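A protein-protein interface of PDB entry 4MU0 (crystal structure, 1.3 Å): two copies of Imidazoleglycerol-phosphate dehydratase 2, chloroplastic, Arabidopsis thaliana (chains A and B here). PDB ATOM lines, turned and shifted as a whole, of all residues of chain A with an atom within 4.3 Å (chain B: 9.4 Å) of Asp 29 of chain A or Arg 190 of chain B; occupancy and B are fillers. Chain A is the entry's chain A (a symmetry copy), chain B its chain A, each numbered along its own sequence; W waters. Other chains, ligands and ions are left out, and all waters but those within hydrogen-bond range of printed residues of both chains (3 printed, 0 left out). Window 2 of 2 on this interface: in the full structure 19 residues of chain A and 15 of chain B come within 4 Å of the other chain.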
ATOM      1  N   ALA A   8      -8.996  14.556  -4.759  1.00  0.00           N
ATOM      2  CA  ALA A   8      -8.598  13.263  -4.196  1.00  0.00           C
ATOM      3  C   ALA A   8      -8.853  12.103  -5.185  1.00  0.00           C
ATOM      4  O   ALA A   8      -9.875  12.062  -5.861  1.00  0.00           O
ATOM      5  CB  ALA A   8      -9.312  13.006  -2.886  1.00  0.00           C
ATOM      6  N   ARG A   9      -7.917  11.162  -5.211  1.00  0.00           N
ATOM      7  CA  ARG A   9      -8.000   9.941  -6.043  1.00  0.00           C
ATOM      8  C   ARG A   9      -8.786   8.846  -5.341  1.00  0.00           C
ATOM      9  O   ARG A   9      -8.317   8.237  -4.396  1.00  0.00           O
ATOM     10  CB  ARG A   9      -6.618   9.463  -6.374  1.00  0.00           C
ATOM     11  CG  ARG A   9      -5.850  10.397  -7.291  1.00  0.00           C
ATOM     12  CD  ARG A   9      -4.384   9.991  -7.379  1.00  0.00           C
ATOM     13  NE  ARG A   9      -3.759  10.119  -6.052  1.00  0.00           N
ATOM     14  CZ  ARG A   9      -2.593   9.574  -5.724  1.00  0.00           C
ATOM     15  NH1 ARG A   9      -1.939   8.794  -6.586  1.00  0.00           N
ATOM     16  NH2 ARG A   9      -2.147   9.735  -4.485  1.00  0.00           N
ATOM     17  N   ASN A  27      -9.777   5.999  -0.901  1.00  0.00           N
ATOM     18  CA  ASN A  27      -9.188   7.320  -1.200  1.00  0.00           C
ATOM     19  C   ASN A  27      -7.695   7.225  -0.963  1.00  0.00           C
ATOM     20  O   ASN A  27      -7.257   7.022   0.162  1.00  0.00           O
ATOM     21  CB  ASN A  27      -9.814   8.400  -0.322  1.00  0.00           C
ATOM     22  CG  ASN A  27      -9.378   9.808  -0.695  1.00  0.00           C
ATOM     23  OD1 ASN A  27      -8.402  10.019  -1.402  1.00  0.00           O
ATOM     24  ND2 ASN A  27     -10.113  10.787  -0.196  1.00  0.00           N
ATOM     25  N   LEU A  28      -6.919   7.339  -2.036  1.00  0.00           N
ATOM     26  CA  LEU A  28      -5.453   7.297  -1.933  1.00  0.00           C
ATOM     27  C   LEU A  28      -4.872   8.507  -1.193  1.00  0.00           C
ATOM     28  O   LEU A  28      -3.762   8.425  -0.660  1.00  0.00           O
ATOM     29  CB  LEU A  28      -4.801   7.201  -3.299  1.00  0.00           C
ATOM     30  CG  LEU A  28      -5.216   6.042  -4.153  1.00  0.00           C
ATOM     31  CD1 LEU A  28      -4.492   6.081  -5.486  1.00  0.00           C
ATOM     32  CD2 LEU A  28      -5.038   4.707  -3.450  1.00  0.00           C
ATOM     33  N   ASP A  29      -5.631   9.606  -1.199  1.00  0.00           N
ATOM     34  CA  ASP A  29      -5.237  10.869  -0.597  1.00  0.00           C
ATOM     35  C   ASP A  29      -6.027  11.123   0.689  1.00  0.00           C
ATOM     36  O   ASP A  29      -6.484  12.232   0.966  1.00  0.00           O
ATOM     37  CB  ASP A  29      -5.406  11.997  -1.618  1.00  0.00           C
ATOM     38  CG  ASP A  29      -4.655  11.724  -2.896  1.00  0.00           C
ATOM     39  OD1 ASP A  29      -3.403  11.601  -2.793  1.00  0.00           O
ATOM     40  OD2 ASP A  29      -5.265  11.575  -3.980  1.00  0.00           O
ATOM     41  N   GLY A  30      -6.168  10.080   1.492  1.00  0.00           N
ATOM     42  CA  GLY A  30      -7.007  10.131   2.657  1.00  0.00           C
ATOM     43  C   GLY A  30      -6.338  10.619   3.926  1.00  0.00           C
ATOM     44  O   GLY A  30      -5.208  11.150   3.933  1.00  0.00           O
ATOM     45  N   LEU A  55      -2.594   5.953   5.525  1.00  0.00           N
ATOM     46  CA  LEU A  55      -3.379   7.185   5.391  1.00  0.00           C
ATOM     47  C   LEU A  55      -4.281   7.122   4.177  1.00  0.00           C
ATOM     48  O   LEU A  55      -4.514   8.093   3.479  1.00  0.00           O
ATOM     49  CB  LEU A  55      -2.521   8.442   5.379  1.00  0.00           C
ATOM     50  CG  LEU A  55      -1.801   8.732   6.700  1.00  0.00           C
ATOM     51  CD1 LEU A  55      -1.032  10.025   6.551  1.00  0.00           C
ATOM     52  CD2 LEU A  55      -2.739   8.740   7.888  1.00  0.00           C
ATOM     53  N   ARG A 182       1.542   3.582   0.579  1.00  0.00           N
ATOM     54  CA  ARG A 182       1.505   5.037   0.734  1.00  0.00           C
ATOM     55  C   ARG A 182       2.636   5.704  -0.048  1.00  0.00           C
ATOM     56  O   ARG A 182       2.425   6.615  -0.854  1.00  0.00           O
ATOM     57  CB  ARG A 182       1.560   5.423   2.204  1.00  0.00           C
ATOM     58  CG  ARG A 182       1.744   6.923   2.404  1.00  0.00           C
ATOM     59  CD  ARG A 182       1.799   7.302   3.868  1.00  0.00           C
ATOM     60  NE  ARG A 182       2.205   8.685   4.004  1.00  0.00           N
ATOM     61  CZ  ARG A 182       2.343   9.348   5.139  1.00  0.00           C
ATOM     62  NH1 ARG A 182       2.111   8.766   6.280  1.00  0.00           N
ATOM     63  NH2 ARG A 182       2.779  10.590   5.100  1.00  0.00           N
ATOM     64  N   GLU A 186       2.013   8.154  -3.445  1.00  0.00           N
ATOM     65  CA  GLU A 186       2.227   9.566  -3.219  1.00  0.00           C
ATOM     66  C   GLU A 186       2.927  10.196  -4.416  1.00  0.00           C
ATOM     67  O   GLU A 186       3.596   9.552  -5.195  1.00  0.00           O
ATOM     68  CB  GLU A 186       3.023   9.797  -1.929  1.00  0.00           C
ATOM     69  CG  GLU A 186       2.138   9.765  -0.683  1.00  0.00           C
ATOM     70  CD  GLU A 186       2.889   9.900   0.639  1.00  0.00           C
ATOM     71  OE1 GLU A 186       4.116   9.705   0.651  1.00  0.00           O
ATOM     72  OE2 GLU A 186       2.232  10.186   1.672  1.00  0.00           O
ATOM     73  N   GLY B  94       1.810  13.244  15.865  1.00  0.00           N
ATOM     74  CA  GLY B  94       2.172  13.743  14.534  1.00  0.00           C
ATOM     75  C   GLY B  94       3.509  13.295  13.981  1.00  0.00           C
ATOM     76  O   GLY B  94       3.924  13.789  12.955  1.00  0.00           O
ATOM     77  N   ILE B  95       4.160  12.335  14.631  1.00  0.00           N
ATOM     78  CA  ILE B  95       5.467  11.838  14.188  1.00  0.00           C
ATOM     79  C   ILE B  95       5.346  10.619  13.270  1.00  0.00           C
ATOM     80  O   ILE B  95       4.315   9.957  13.194  1.00  0.00           O
ATOM     81  CB  ILE B  95       6.403  11.552  15.373  1.00  0.00           C
ATOM     82  CG1 ILE B  95       5.888  10.383  16.210  1.00  0.00           C
ATOM     83  CG2 ILE B  95       6.593  12.823  16.222  1.00  0.00           C
ATOM     84  CD1 ILE B  95       6.846   9.920  17.285  1.00  0.00           C
ATOM     85  N   ASN B  96       6.416  10.337  12.549  1.00  0.00           N
ATOM     86  CA  ASN B  96       6.420   9.164  11.668  1.00  0.00           C
ATOM     87  C   ASN B  96       6.271   7.855  12.452  1.00  0.00           C
ATOM     88  O   ASN B  96       5.674   6.902  11.936  1.00  0.00           O
ATOM     89  CB  ASN B  96       7.703   9.128  10.851  1.00  0.00           C
ATOM     90  CG  ASN B  96       7.715  10.165   9.734  1.00  0.00           C
ATOM     91  OD1 ASN B  96       6.707  10.377   9.061  1.00  0.00           O
ATOM     92  ND2 ASN B  96       8.879  10.791   9.524  1.00  0.00           N
ATOM     93  N   GLU B 186      10.820  12.397  13.423  1.00  0.00           N
ATOM     94  CA  GLU B 186      10.446  13.534  12.611  1.00  0.00           C
ATOM     95  C   GLU B 186       8.936  13.568  12.409  1.00  0.00           C
ATOM     96  O   GLU B 186       8.241  12.581  12.506  1.00  0.00           O
ATOM     97  CB  GLU B 186      11.183  13.511  11.267  1.00  0.00           C
ATOM     98  CG  GLU B 186      12.596  14.087  11.366  1.00  0.00           C
ATOM     99  CD  GLU B 186      13.411  14.008  10.077  1.00  0.00           C
ATOM    100  OE1 GLU B 186      13.035  13.234   9.180  1.00  0.00           O
ATOM    101  OE2 GLU B 186      14.445  14.716   9.981  1.00  0.00           O
ATOM    102  N   SER B 187       8.450  14.765  12.091  1.00  0.00           N
ATOM    103  CA  SER B 187       7.058  15.007  11.748  1.00  0.00           C
ATOM    104  C   SER B 187       6.653  14.225  10.515  1.00  0.00           C
ATOM    105  O   SER B 187       7.372  14.217   9.521  1.00  0.00           O
ATOM    106  CB  SER B 187       6.824  16.498  11.470  1.00  0.00           C
ATOM    107  OG  SER B 187       5.493  16.718  11.044  1.00  0.00           O
ATOM    108  N   ASP B 188       5.478  13.611  10.570  1.00  0.00           N
ATOM    109  CA  ASP B 188       4.858  13.041   9.382  1.00  0.00           C
ATOM    110  C   ASP B 188       4.099  14.222   8.746  1.00  0.00           C
ATOM    111  O   ASP B 188       3.197  14.763   9.372  1.00  0.00           O
ATOM    112  CB  ASP B 188       3.910  11.906   9.801  1.00  0.00           C
ATOM    113  CG  ASP B 188       3.234  11.239   8.640  1.00  0.00           C
ATOM    114  OD1 ASP B 188       2.934  11.948   7.636  1.00  0.00           O
ATOM    115  OD2 ASP B 188       2.974  10.013   8.725  1.00  0.00           O
ATOM    116  N   PRO B 189       4.425  14.599   7.500  1.00  0.00           N
ATOM    117  CA  PRO B 189       3.810  15.810   6.934  1.00  0.00           C
ATOM    118  C   PRO B 189       2.291  15.710   6.688  1.00  0.00           C
ATOM    119  O   PRO B 189       1.617  16.738   6.454  1.00  0.00           O
ATOM    120  CB  PRO B 189       4.540  15.985   5.597  1.00  0.00           C
ATOM    121  CG  PRO B 189       4.987  14.607   5.230  1.00  0.00           C
ATOM    122  CD  PRO B 189       5.356  13.974   6.562  1.00  0.00           C
ATOM    123  N   ARG B 190       1.757  14.493   6.718  1.00  0.00           N
ATOM    124  CA  ARG B 190       0.310  14.278   6.558  1.00  0.00           C
ATOM    125  C   ARG B 190      -0.421  14.021   7.887  1.00  0.00           C
ATOM    126  O   ARG B 190      -1.613  13.733   7.893  1.00  0.00           O
ATOM    127  CB  ARG B 190       0.020  13.144   5.554  1.00  0.00           C
ATOM    128  CG  ARG B 190       0.379  13.537   4.129  1.00  0.00           C
ATOM    129  CD  ARG B 190       0.239  12.398   3.124  1.00  0.00           C
ATOM    130  NE  ARG B 190      -1.147  11.948   3.024  1.00  0.00           N
ATOM    131  CZ  ARG B 190      -1.522  10.818   2.443  1.00  0.00           C
ATOM    132  NH1 ARG B 190      -0.616  10.006   1.914  1.00  0.00           N
ATOM    133  NH2 ARG B 190      -2.807  10.488   2.420  1.00  0.00           N
ATOM    134  N   ARG B 191       0.308  14.139   9.001  1.00  0.00           N
ATOM    135  CA  ARG B 191      -0.265  13.970  10.349  1.00  0.00           C
ATOM    136  C   ARG B 191      -0.216  15.268  11.159  1.00  0.00           C
ATOM    137  O   ARG B 191      -0.442  15.221  12.356  1.00  0.00           O
ATOM    138  CB  ARG B 191       0.409  12.807  11.119  1.00  0.00           C
ATOM    139  CG  ARG B 191       0.228  11.469  10.432  1.00  0.00           C
ATOM    140  CD  ARG B 191       0.888  10.340  11.211  1.00  0.00           C
ATOM    141  NE  ARG B 191       0.891   9.090  10.434  1.00  0.00           N
ATOM    142  CZ  ARG B 191      -0.057   8.160  10.452  1.00  0.00           C
ATOM    143  NH1 ARG B 191      -1.127   8.323  11.211  1.00  0.00           N
ATOM    144  NH2 ARG B 191       0.067   7.073   9.684  1.00  0.00           N
HETATM  145  O   HOH W   1      -3.468  13.586   3.911  1.00  0.00           O
HETATM  146  O   HOH W   2       1.960   6.296   7.550  1.00  0.00           O
HETATM  147  O   HOH W   3      -1.944   7.656   1.346  1.00  0.00           O
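Arg 190 of chain B touches Leu 28 of chain A (NH2 to O, 3.8 Å). Asp 29 of chain A touches Arg 190 of chain B (C to NH2, 3.7 Å). CD2 of Leu 55 of chain A touches NH1 of Arg 191 of chain B (3.7 Å). NH2 of Arg 182 of chain A touches CD of Arg 190 of chain B, at 3.7 Å.
Of the 9 printed residues of chain A, 6 touch a printed residue of chain B. Hydrophobic or aromatic side chains of chain A within 4 Å of the printed part of chain B: Leu 55. Among the printed residues, Asp or Glu carboxylates within 4 Å of a Lys or Arg side-chain nitrogen of the other chain: Arg 182 of chain A with Asp 188 of chain B and Glu 186 of chain A with Arg 190 of chain B.
The side-chain carboxylate of Asp 188 of chain B lies within salt-bridge range of the guanidinium group of Arg 182 of chain A (2.9 Å). NH2 of Arg 190 of chain B sits at hydrogen-bond distance from O of Gly 30 of chain A (2.9 Å). O of Leu 55 of chain A lies within hydrogen-bond range of NH2 of Arg 190 of chain B (3.1 Å). The guanidinium group (NH1) of Arg 190 of chain B lies within salt-bridge range of the side-chain carboxylate (OE2) of Glu 186 of chain A (2.9 Å).
Asp 29 of chain A touches just one residue of chain B: Arg 190. No residue of chain B comes within 4 Å of Arg 9 of chain A. Of the printed residues of chain B, Glu 186 of chain A touches Arg 190 (2.9 Å). Of the printed residues of chain A, Arg 191 of chain B touches Leu 55 (3.7 Å). Of the printed residues of chain B, Arg 182 of chain A touches Asp 188 (2.9 Å) and Arg 190 (3.7 Å). Of the printed residues of chain A, Asp 188 of chain B touches Arg 182 (2.9 Å). Of the printed residues of chain B, Leu 55 of chain A touches Arg 190 (3.1 Å) and Arg 191 (3.7 Å). The nearest printed residue of chain A that does not touch Arg 190 of chain B is Asn 27 of chain A (6.1 Å). The nearest printed residue of chain B that does not touch Leu 55 of chain A is Asp 188 of chain B (4.5 Å).
N of Arg 190 of chain B lies within hydrogen-bond range of OD1 of Asp 188 of chain B (3.0 Å). The backbone carbonyl oxygen of Arg 9 of chain A lies within hydrogen-bond range of the backbone NH of Leu 28 of chain A (2.9 Å). The guanidinium group (NH2) of Arg 9 of chain A lies within salt-bridge range of the side-chain carboxylate (OD1) of Asp 29 of chain A (2.8 Å). The backbone NH (N) of Asp 29 of chain A sits at hydrogen-bond distance from the side-chain amide oxygen (OD1) of Asn 27 of chain A (2.8 Å). The backbone NH (N) of Gly 30 of chain A lies close to the backbone carbonyl oxygen (O) of Leu 55 of chain A, at 3.3 Å. The side-chain carboxylate (OE2) of Glu 186 of chain A is in salt-bridge range of the guanidinium group (NE) of Arg 182 of chain A, 2.8 Å away.
Position printed for both chains: 186.
Water W3 lies within hydrogen-bond range of NH1 of Arg 190 of chain B (2.8 Å), O of Leu 28 of chain A (2.8 Å) and O of Leu 55 of chain A (3.4 Å). Water W2 lies within hydrogen-bond range of NH1 of Arg 182 of chain A (2.8 Å) and NH2 of Arg 191 of chain B (3.0 Å). Water W1 bridges NE of Arg 190 of chain B (3.0 Å) and O of Gly 30 of chain A (3.0 Å).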
